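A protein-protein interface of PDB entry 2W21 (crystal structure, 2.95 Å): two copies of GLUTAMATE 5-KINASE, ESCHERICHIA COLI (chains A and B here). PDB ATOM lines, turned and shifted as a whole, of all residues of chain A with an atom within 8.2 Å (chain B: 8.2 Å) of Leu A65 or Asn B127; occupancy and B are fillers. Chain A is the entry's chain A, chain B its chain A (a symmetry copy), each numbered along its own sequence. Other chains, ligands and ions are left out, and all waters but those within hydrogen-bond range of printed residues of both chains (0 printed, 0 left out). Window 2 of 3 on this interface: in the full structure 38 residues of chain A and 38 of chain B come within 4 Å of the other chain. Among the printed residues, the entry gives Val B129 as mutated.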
ATOM      1  N   GLY A  56      17.138  21.613 -14.532  1.00  0.00           N
ATOM      2  CA  GLY A  56      17.887  20.598 -15.266  1.00  0.00           C
ATOM      3  C   GLY A  56      19.279  20.364 -14.705  1.00  0.00           C
ATOM      4  O   GLY A  56      19.768  19.224 -14.773  1.00  0.00           O
ATOM      5  N   ARG A  57      19.924  21.426 -14.164  1.00  0.00           N
ATOM      6  CA  ARG A  57      21.282  21.295 -13.578  1.00  0.00           C
ATOM      7  C   ARG A  57      21.176  20.508 -12.308  1.00  0.00           C
ATOM      8  O   ARG A  57      21.898  19.522 -12.104  1.00  0.00           O
ATOM      9  CB  ARG A  57      21.961  22.619 -13.224  1.00  0.00           C
ATOM     10  CG  ARG A  57      22.006  23.669 -14.300  1.00  0.00           C
ATOM     11  CD  ARG A  57      22.977  24.796 -14.001  1.00  0.00           C
ATOM     12  NE  ARG A  57      24.107  24.581 -14.874  1.00  0.00           N
ATOM     13  CZ  ARG A  57      24.352  25.311 -15.968  1.00  0.00           C
ATOM     14  NH1 ARG A  57      23.548  26.338 -16.263  1.00  0.00           N
ATOM     15  NH2 ARG A  57      25.410  25.035 -16.757  1.00  0.00           N
ATOM     16  N   LEU A  60      20.398  16.756 -12.828  1.00  0.00           N
ATOM     17  CA  LEU A  60      21.496  15.991 -13.431  1.00  0.00           C
ATOM     18  C   LEU A  60      22.765  15.994 -12.571  1.00  0.00           C
ATOM     19  O   LEU A  60      23.826  15.514 -13.010  1.00  0.00           O
ATOM     20  CB  LEU A  60      21.818  16.536 -14.813  1.00  0.00           C
ATOM     21  CG  LEU A  60      20.833  16.317 -15.951  1.00  0.00           C
ATOM     22  CD1 LEU A  60      21.311  17.143 -17.102  1.00  0.00           C
ATOM     23  CD2 LEU A  60      20.714  14.853 -16.378  1.00  0.00           C
ATOM     24  N   TYR A  62      24.467  18.780 -11.345  1.00  0.00           N
ATOM     25  CA  TYR A  62      25.423  19.791 -11.775  1.00  0.00           C
ATOM     26  C   TYR A  62      26.614  19.229 -12.569  1.00  0.00           C
ATOM     27  O   TYR A  62      27.777  19.347 -12.136  1.00  0.00           O
ATOM     28  CB  TYR A  62      25.864  20.620 -10.567  1.00  0.00           C
ATOM     29  CG  TYR A  62      24.689  20.970  -9.678  1.00  0.00           C
ATOM     30  CD1 TYR A  62      24.178  20.030  -8.767  1.00  0.00           C
ATOM     31  CD2 TYR A  62      24.054  22.219  -9.768  1.00  0.00           C
ATOM     32  CE1 TYR A  62      23.100  20.326  -7.971  1.00  0.00           C
ATOM     33  CE2 TYR A  62      22.959  22.511  -8.970  1.00  0.00           C
ATOM     34  CZ  TYR A  62      22.504  21.553  -8.082  1.00  0.00           C
ATOM     35  OH  TYR A  62      21.428  21.800  -7.286  1.00  0.00           O
ATOM     36  N   PRO A  63      26.336  18.604 -13.738  1.00  0.00           N
ATOM     37  CA  PRO A  63      27.424  18.035 -14.558  1.00  0.00           C
ATOM     38  C   PRO A  63      28.224  19.113 -15.263  1.00  0.00           C
ATOM     39  O   PRO A  63      27.730  20.231 -15.442  1.00  0.00           O
ATOM     40  CB  PRO A  63      26.676  17.210 -15.597  1.00  0.00           C
ATOM     41  CG  PRO A  63      25.370  17.930 -15.729  1.00  0.00           C
ATOM     42  CD  PRO A  63      25.017  18.381 -14.352  1.00  0.00           C
ATOM     43  N   GLU A  64      29.450  18.766 -15.659  1.00  0.00           N
ATOM     44  CA  GLU A  64      30.336  19.678 -16.407  1.00  0.00           C
ATOM     45  C   GLU A  64      30.062  19.568 -17.902  1.00  0.00           C
ATOM     46  O   GLU A  64      30.222  18.485 -18.474  1.00  0.00           O
ATOM     47  CB  GLU A  64      31.823  19.378 -16.096  1.00  0.00           C
ATOM     48  CG  GLU A  64      32.462  20.328 -15.024  1.00  0.00           C
ATOM     49  CD  GLU A  64      32.404  21.817 -15.455  1.00  0.00           C
ATOM     50  OE1 GLU A  64      31.519  22.566 -14.950  1.00  0.00           O
ATOM     51  OE2 GLU A  64      33.222  22.219 -16.327  1.00  0.00           O
ATOM     52  N   LEU A  65      29.612  20.664 -18.520  1.00  0.00           N
ATOM     53  CA  LEU A  65      29.213  20.612 -19.937  1.00  0.00           C
ATOM     54  C   LEU A  65      29.849  21.731 -20.762  1.00  0.00           C
ATOM     55  O   LEU A  65      30.060  22.818 -20.240  1.00  0.00           O
ATOM     56  CB  LEU A  65      27.686  20.696 -20.081  1.00  0.00           C
ATOM     57  CG  LEU A  65      26.809  19.732 -19.300  1.00  0.00           C
ATOM     58  CD1 LEU A  65      25.439  20.280 -19.197  1.00  0.00           C
ATOM     59  CD2 LEU A  65      26.765  18.392 -19.938  1.00  0.00           C
ATOM     60  N   PRO A  66      30.146  21.468 -22.062  1.00  0.00           N
ATOM     61  CA  PRO A  66      30.628  22.538 -22.962  1.00  0.00           C
ATOM     62  C   PRO A  66      29.675  23.738 -23.034  1.00  0.00           C
ATOM     63  O   PRO A  66      28.469  23.569 -22.934  1.00  0.00           O
ATOM     64  CB  PRO A  66      30.727  21.843 -24.332  1.00  0.00           C
ATOM     65  CG  PRO A  66      30.051  20.517 -24.195  1.00  0.00           C
ATOM     66  CD  PRO A  66      30.080  20.155 -22.744  1.00  0.00           C
ATOM     67  N   ALA A  67      30.193  24.946 -23.196  1.00  0.00           N
ATOM     68  CA  ALA A  67      29.307  26.085 -23.346  1.00  0.00           C
ATOM     69  C   ALA A  67      28.699  26.138 -24.766  1.00  0.00           C
ATOM     70  O   ALA A  67      28.713  27.183 -25.412  1.00  0.00           O
ATOM     71  CB  ALA A  67      30.038  27.397 -22.990  1.00  0.00           C
ATOM     72  N   THR A  68      28.181  25.009 -25.255  1.00  0.00           N
ATOM     73  CA  THR A  68      27.411  24.980 -26.491  1.00  0.00           C
ATOM     74  C   THR A  68      26.036  25.559 -26.194  1.00  0.00           C
ATOM     75  O   THR A  68      25.656  25.736 -25.023  1.00  0.00           O
ATOM     76  CB  THR A  68      27.125  23.545 -26.962  1.00  0.00           C
ATOM     77  OG1 THR A  68      28.148  22.659 -26.513  1.00  0.00           O
ATOM     78  CG2 THR A  68      26.934  23.443 -28.547  1.00  0.00           C
ATOM     79  N   ALA A  70      23.781  23.525 -27.338  1.00  0.00           N
ATOM     80  CA  ALA A  70      23.281  22.183 -26.983  1.00  0.00           C
ATOM     81  C   ALA A  70      23.339  21.838 -25.492  1.00  0.00           C
ATOM     82  O   ALA A  70      22.675  20.910 -25.034  1.00  0.00           O
ATOM     83  CB  ALA A  70      23.959  21.097 -27.806  1.00  0.00           C
ATOM     84  N   SER A  71      24.133  22.559 -24.724  1.00  0.00           N
ATOM     85  CA  SER A  71      24.144  22.283 -23.306  1.00  0.00           C
ATOM     86  C   SER A  71      23.006  23.025 -22.603  1.00  0.00           C
ATOM     87  O   SER A  71      22.369  22.455 -21.684  1.00  0.00           O
ATOM     88  CB  SER A  71      25.498  22.597 -22.688  1.00  0.00           C
ATOM     89  OG  SER A  71      26.491  21.840 -23.350  1.00  0.00           O
ATOM     90  N   LYS A  72      22.729  24.264 -23.031  1.00  0.00           N
ATOM     91  CA  LYS A  72      21.615  24.991 -22.449  1.00  0.00           C
ATOM     92  C   LYS A  72      20.372  24.197 -22.820  1.00  0.00           C
ATOM     93  O   LYS A  72      19.507  23.949 -21.978  1.00  0.00           O
ATOM     94  CB  LYS A  72      21.532  26.469 -22.915  1.00  0.00           C
ATOM     95  N   GLN A  73      20.326  23.712 -24.047  1.00  0.00           N
ATOM     96  CA  GLN A  73      19.138  23.021 -24.498  1.00  0.00           C
ATOM     97  C   GLN A  73      18.859  21.696 -23.807  1.00  0.00           C
ATOM     98  O   GLN A  73      17.737  21.479 -23.394  1.00  0.00           O
ATOM     99  CB  GLN A  73      19.118  22.893 -26.009  1.00  0.00           C
ATOM    100  CG  GLN A  73      18.817  24.236 -26.630  1.00  0.00           C
ATOM    101  CD  GLN A  73      18.704  24.194 -28.131  1.00  0.00           C
ATOM    102  OE1 GLN A  73      18.235  25.158 -28.749  1.00  0.00           O
ATOM    103  NE2 GLN A  73      19.134  23.093 -28.738  1.00  0.00           N
ATOM    104  N   LEU A  74      19.858  20.823 -23.659  1.00  0.00           N
ATOM    105  CA  LEU A  74      19.642  19.553 -22.930  1.00  0.00           C
ATOM    106  C   LEU A  74      19.317  19.814 -21.448  1.00  0.00           C
ATOM    107  O   LEU A  74      18.445  19.130 -20.876  1.00  0.00           O
ATOM    108  CB  LEU A  74      20.805  18.569 -23.083  1.00  0.00           C
ATOM    109  CG  LEU A  74      22.078  18.696 -22.237  1.00  0.00           C
ATOM    110  CD1 LEU A  74      21.976  17.970 -20.922  1.00  0.00           C
ATOM    111  CD2 LEU A  74      23.207  18.077 -23.019  1.00  0.00           C
ATOM    112  N   LEU A  75      19.988  20.796 -20.826  1.00  0.00           N
ATOM    113  CA  LEU A  75      19.597  21.185 -19.469  1.00  0.00           C
ATOM    114  C   LEU A  75      18.119  21.536 -19.485  1.00  0.00           C
ATOM    115  O   LEU A  75      17.357  20.988 -18.711  1.00  0.00           O
ATOM    116  CB  LEU A  75      20.449  22.331 -18.923  1.00  0.00           C
ATOM    117  CG  LEU A  75      21.924  21.990 -18.709  1.00  0.00           C
ATOM    118  CD1 LEU A  75      22.688  23.231 -18.330  1.00  0.00           C
ATOM    119  CD2 LEU A  75      22.115  20.892 -17.659  1.00  0.00           C
ATOM    120  N   ALA A  76      17.720  22.407 -20.411  1.00  0.00           N
ATOM    121  CA  ALA A  76      16.318  22.824 -20.562  1.00  0.00           C
ATOM    122  C   ALA A  76      15.348  21.677 -20.842  1.00  0.00           C
ATOM    123  O   ALA A  76      14.248  21.678 -20.338  1.00  0.00           O
ATOM    124  CB  ALA A  76      16.188  23.865 -21.635  1.00  0.00           C
ATOM    125  N   VAL A  78      15.683  18.602 -19.761  1.00  0.00           N
ATOM    126  CA  VAL A  78      15.532  17.832 -18.544  1.00  0.00           C
ATOM    127  C   VAL A  78      14.782  18.681 -17.510  1.00  0.00           C
ATOM    128  O   VAL A  78      13.772  18.244 -16.960  1.00  0.00           O
ATOM    129  CB  VAL A  78      16.881  17.322 -18.062  1.00  0.00           C
ATOM    130  CG1 VAL A  78      16.810  16.848 -16.649  1.00  0.00           C
ATOM    131  CG2 VAL A  78      17.343  16.198 -18.951  1.00  0.00           C
ATOM    132  N   HIS B  39      19.389   0.380 -22.263  1.00  0.00           N
ATOM    133  CA  HIS B  39      20.127   1.523 -21.768  1.00  0.00           C
ATOM    134  C   HIS B  39      21.258   1.048 -20.867  1.00  0.00           C
ATOM    135  O   HIS B  39      22.389   1.504 -20.982  1.00  0.00           O
ATOM    136  CB  HIS B  39      19.197   2.413 -20.993  1.00  0.00           C
ATOM    137  CG  HIS B  39      19.782   3.734 -20.649  1.00  0.00           C
ATOM    138  ND1 HIS B  39      20.328   3.996 -19.418  1.00  0.00           N
ATOM    139  CD2 HIS B  39      19.869   4.882 -21.355  1.00  0.00           C
ATOM    140  CE1 HIS B  39      20.726   5.254 -19.372  1.00  0.00           C
ATOM    141  NE2 HIS B  39      20.453   5.816 -20.533  1.00  0.00           N
ATOM    142  N   ARG B  44      21.722   3.547 -26.789  1.00  0.00           N
ATOM    143  CA  ARG B  44      21.190   4.893 -26.793  1.00  0.00           C
ATOM    144  C   ARG B  44      19.730   4.815 -27.229  1.00  0.00           C
ATOM    145  O   ARG B  44      19.447   4.221 -28.289  1.00  0.00           O
ATOM    146  CB  ARG B  44      21.984   5.741 -27.774  1.00  0.00           C
ATOM    147  CG  ARG B  44      23.367   6.086 -27.283  1.00  0.00           C
ATOM    148  CD  ARG B  44      24.337   6.459 -28.416  1.00  0.00           C
ATOM    149  NE  ARG B  44      25.029   7.692 -28.038  1.00  0.00           N
ATOM    150  CZ  ARG B  44      24.932   8.855 -28.690  1.00  0.00           C
ATOM    151  NH1 ARG B  44      24.202   8.936 -29.806  1.00  0.00           N
ATOM    152  NH2 ARG B  44      25.582   9.938 -28.239  1.00  0.00           N
ATOM    153  N   ILE B  96      16.967   6.233 -14.951  1.00  0.00           N
ATOM    154  CA  ILE B  96      17.307   6.875 -16.215  1.00  0.00           C
ATOM    155  C   ILE B  96      16.556   8.196 -16.295  1.00  0.00           C
ATOM    156  O   ILE B  96      15.341   8.226 -16.053  1.00  0.00           O
ATOM    157  CB  ILE B  96      16.787   6.030 -17.355  1.00  0.00           C
ATOM    158  CG1 ILE B  96      17.364   4.601 -17.292  1.00  0.00           C
ATOM    159  CG2 ILE B  96      17.037   6.751 -18.664  1.00  0.00           C
ATOM    160  CD1 ILE B  96      16.782   3.633 -18.283  1.00  0.00           C
ATOM    161  N   HIS B  97      17.259   9.278 -16.646  1.00  0.00           N
ATOM    162  CA  HIS B  97      16.615  10.616 -16.830  1.00  0.00           C
ATOM    163  C   HIS B  97      16.017  10.801 -18.229  1.00  0.00           C
ATOM    164  O   HIS B  97      16.352  10.074 -19.180  1.00  0.00           O
ATOM    165  CB  HIS B  97      17.571  11.765 -16.570  1.00  0.00           C
ATOM    166  CG  HIS B  97      18.310  11.654 -15.279  1.00  0.00           C
ATOM    167  ND1 HIS B  97      17.690  11.766 -14.050  1.00  0.00           N
ATOM    168  CD2 HIS B  97      19.624  11.428 -15.017  1.00  0.00           C
ATOM    169  CE1 HIS B  97      18.588  11.622 -13.088  1.00  0.00           C
ATOM    170  NE2 HIS B  97      19.769  11.407 -13.648  1.00  0.00           N
ATOM    171  N   ASP B 119      21.979  18.511 -32.641  1.00  0.00           N
ATOM    172  CA  ASP B 119      23.074  18.683 -31.696  1.00  0.00           C
ATOM    173  C   ASP B 119      22.614  18.315 -30.307  1.00  0.00           C
ATOM    174  O   ASP B 119      23.361  17.712 -29.500  1.00  0.00           O
ATOM    175  CB  ASP B 119      23.553  20.129 -31.693  1.00  0.00           C
ATOM    176  CG  ASP B 119      24.357  20.490 -32.928  1.00  0.00           C
ATOM    177  OD1 ASP B 119      24.822  19.568 -33.688  1.00  0.00           O
ATOM    178  OD2 ASP B 119      24.519  21.727 -33.122  1.00  0.00           O
ATOM    179  N   THR B 120      21.367  18.702 -30.046  1.00  0.00           N
ATOM    180  CA  THR B 120      20.777  18.608 -28.740  1.00  0.00           C
ATOM    181  C   THR B 120      20.409  17.178 -28.492  1.00  0.00           C
ATOM    182  O   THR B 120      20.705  16.650 -27.434  1.00  0.00           O
ATOM    183  CB  THR B 120      19.611  19.525 -28.684  1.00  0.00           C
ATOM    184  OG1 THR B 120      20.138  20.846 -28.725  1.00  0.00           O
ATOM    185  CG2 THR B 120      18.857  19.381 -27.417  1.00  0.00           C
ATOM    186  N   LEU B 121      19.832  16.527 -29.488  1.00  0.00           N
ATOM    187  CA  LEU B 121      19.528  15.136 -29.357  1.00  0.00           C
ATOM    188  C   LEU B 121      20.773  14.391 -28.966  1.00  0.00           C
ATOM    189  O   LEU B 121      20.734  13.523 -28.096  1.00  0.00           O
ATOM    190  CB  LEU B 121      18.974  14.584 -30.649  1.00  0.00           C
ATOM    191  CG  LEU B 121      17.528  14.120 -30.713  1.00  0.00           C
ATOM    192  CD1 LEU B 121      16.581  15.052 -30.021  1.00  0.00           C
ATOM    193  CD2 LEU B 121      17.143  13.997 -32.156  1.00  0.00           C
ATOM    194  N   ARG B 122      21.901  14.740 -29.567  1.00  0.00           N
ATOM    195  CA  ARG B 122      23.108  13.951 -29.330  1.00  0.00           C
ATOM    196  C   ARG B 122      23.715  14.306 -28.001  1.00  0.00           C
ATOM    197  O   ARG B 122      24.253  13.458 -27.323  1.00  0.00           O
ATOM    198  CB  ARG B 122      24.099  14.149 -30.452  1.00  0.00           C
ATOM    199  CG  ARG B 122      23.447  14.008 -31.777  1.00  0.00           C
ATOM    200  CD  ARG B 122      24.192  13.097 -32.668  1.00  0.00           C
ATOM    201  NE  ARG B 122      23.654  13.282 -34.009  1.00  0.00           N
ATOM    202  CZ  ARG B 122      24.114  12.686 -35.109  1.00  0.00           C
ATOM    203  NH1 ARG B 122      25.151  11.841 -35.015  1.00  0.00           N
ATOM    204  NH2 ARG B 122      23.535  12.938 -36.294  1.00  0.00           N
ATOM    205  N   ALA B 123      23.608  15.569 -27.618  1.00  0.00           N
ATOM    206  CA  ALA B 123      24.053  15.999 -26.305  1.00  0.00           C
ATOM    207  C   ALA B 123      23.286  15.197 -25.270  1.00  0.00           C
ATOM    208  O   ALA B 123      23.902  14.582 -24.392  1.00  0.00           O
ATOM    209  CB  ALA B 123      23.835  17.495 -26.131  1.00  0.00           C
ATOM    210  N   LEU B 124      21.950  15.145 -25.409  1.00  0.00           N
ATOM    211  CA  LEU B 124      21.100  14.305 -24.532  1.00  0.00           C
ATOM    212  C   LEU B 124      21.643  12.895 -24.400  1.00  0.00           C
ATOM    213  O   LEU B 124      22.026  12.500 -23.302  1.00  0.00           O
ATOM    214  CB  LEU B 124      19.632  14.283 -24.956  1.00  0.00           C
ATOM    215  CG  LEU B 124      18.908  15.569 -24.569  1.00  0.00           C
ATOM    216  CD1 LEU B 124      17.626  15.705 -25.336  1.00  0.00           C
ATOM    217  CD2 LEU B 124      18.653  15.660 -23.076  1.00  0.00           C
ATOM    218  N   LEU B 125      21.717  12.155 -25.504  1.00  0.00           N
ATOM    219  CA  LEU B 125      22.192  10.772 -25.431  1.00  0.00           C
ATOM    220  C   LEU B 125      23.601  10.615 -24.819  1.00  0.00           C
ATOM    221  O   LEU B 125      23.835   9.768 -23.953  1.00  0.00           O
ATOM    222  CB  LEU B 125      22.106  10.124 -26.800  1.00  0.00           C
ATOM    223  CG  LEU B 125      20.699  10.126 -27.357  1.00  0.00           C
ATOM    224  CD1 LEU B 125      20.745   9.855 -28.831  1.00  0.00           C
ATOM    225  CD2 LEU B 125      19.900   9.048 -26.654  1.00  0.00           C
ATOM    226  N   ASP B 126      24.517  11.456 -25.284  1.00  0.00           N
ATOM    227  CA  ASP B 126      25.871  11.558 -24.748  1.00  0.00           C
ATOM    228  C   ASP B 126      25.856  11.582 -23.247  1.00  0.00           C
ATOM    229  O   ASP B 126      26.724  10.977 -22.653  1.00  0.00           O
ATOM    230  CB  ASP B 126      26.566  12.855 -25.185  1.00  0.00           C
ATOM    231  CG  ASP B 126      27.110  12.790 -26.574  1.00  0.00           C
ATOM    232  OD1 ASP B 126      27.505  13.870 -27.060  1.00  0.00           O
ATOM    233  OD2 ASP B 126      27.126  11.692 -27.182  1.00  0.00           O
ATOM    234  N   ASN B 127      24.906  12.299 -22.642  1.00  0.00           N
ATOM    235  CA  ASN B 127      24.858  12.390 -21.203  1.00  0.00           C
ATOM    236  C   ASN B 127      23.854  11.437 -20.603  1.00  0.00           C
ATOM    237  O   ASN B 127      23.302  11.709 -19.554  1.00  0.00           O
ATOM    238  CB  ASN B 127      24.544  13.803 -20.796  1.00  0.00           C
ATOM    239  CG  ASN B 127      25.592  14.783 -21.263  1.00  0.00           C
ATOM    240  OD1 ASN B 127      26.375  15.286 -20.469  1.00  0.00           O
ATOM    241  ND2 ASN B 127      25.612  15.069 -22.549  1.00  0.00           N
ATOM    242  N   ASN B 128      23.612  10.326 -21.292  1.00  0.00           N
ATOM    243  CA  ASN B 128      22.745   9.217 -20.815  1.00  0.00           C
ATOM    244  C   ASN B 128      21.233   9.443 -20.657  1.00  0.00           C
ATOM    245  O   ASN B 128      20.529   8.580 -20.110  1.00  0.00           O
ATOM    246  CB  ASN B 128      23.316   8.578 -19.547  1.00  0.00           C
ATOM    247  CG  ASN B 128      24.435   7.628 -19.861  1.00  0.00           C
ATOM    248  OD1 ASN B 128      25.596   8.043 -19.919  1.00  0.00           O
ATOM    249  ND2 ASN B 128      24.102   6.356 -20.140  1.00  0.00           N
ATOM    250  N   VAL B 129      20.747  10.579 -21.155  1.00  0.00           N
ATOM    251  CA  VAL B 129      19.363  10.940 -21.005  1.00  0.00           C
ATOM    252  C   VAL B 129      18.565  10.355 -22.155  1.00  0.00           C
ATOM    253  O   VAL B 129      19.039  10.355 -23.273  1.00  0.00           O
ATOM    254  CB  VAL B 129      19.235  12.437 -21.032  1.00  0.00           C
ATOM    255  CG1 VAL B 129      17.790  12.834 -20.829  1.00  0.00           C
ATOM    256  CG2 VAL B 129      20.121  13.078 -19.953  1.00  0.00           C
ATOM    257  N   VAL B 130      17.371   9.830 -21.890  1.00  0.00           N
ATOM    258  CA  VAL B 130      16.432   9.439 -22.958  1.00  0.00           C
ATOM    259  C   VAL B 130      15.589  10.664 -23.402  1.00  0.00           C
ATOM    260  O   VAL B 130      14.836  11.230 -22.592  1.00  0.00           O
ATOM    261  CB  VAL B 130      15.490   8.324 -22.462  1.00  0.00           C
ATOM    262  CG1 VAL B 130      14.549   7.899 -23.536  1.00  0.00           C
ATOM    263  CG2 VAL B 130      16.303   7.136 -22.001  1.00  0.00           C
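Leu A65 touches just one residue of chain B: Asn B127 (3.2 Å).
No residue of chain B comes within 4 Å of Pro A66.
Printed residues of chain A within 4 Å of His B97: Leu A60.
Printed residues of chain B within 4 Å of Gln A73: Thr B120 (2.5 Å).
Pro A63 touches none of the printed residues of chain B.
The side-chain hydroxyl of Thr B120 is in hydrogen-bond range of the side-chain amide nitrogen of Gln A73 (2.5 Å).
Printed residues of chain B that touch a printed residue of chain A: His B97, Asp B119, Thr B120, Ala B123, Leu B124, Asn B127 and Val B129.
Among the printed residues, no Asp or Glu carboxylate lies within 4 Å of a Lys or Arg side-chain nitrogen of the other chain.
No position is printed for both chains.
Of the 10 pairs that touch across the chains among the printed residues, none has its exchanged pair printed and touching as well.
The backbone carbonyl oxygen (O) of His B97 sits at hydrogen-bond distance from the backbone NH (N) of Val B130, at 2.9 Å.
The backbone carbonyl oxygen (O) of Ala B123 lies within hydrogen-bond range of the side-chain amide nitrogen (ND2) of Asn B127 (2.6 Å).
O of Leu B124 sits at hydrogen-bond distance from N of Val B129, at 3.2 Å.
Among the printed residues, pairs that only touch across the chains: Leu A65 with Asn B127 (3.2 Å), Leu A74 with Ala B123 (3.2 Å), Leu A74 with Leu B124 (3.6 Å), Ala A70 with Ala B123 (3.8 Å), Ala A70 with Asp B119 (3.8 Å), Ala A70 with Thr B120 (3.8 Å), Leu A60 with His B97 (3.8 Å), Val A78 with Val B129 (3.9 Å) and Leu A74 with Asn B127 (3.9 Å).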
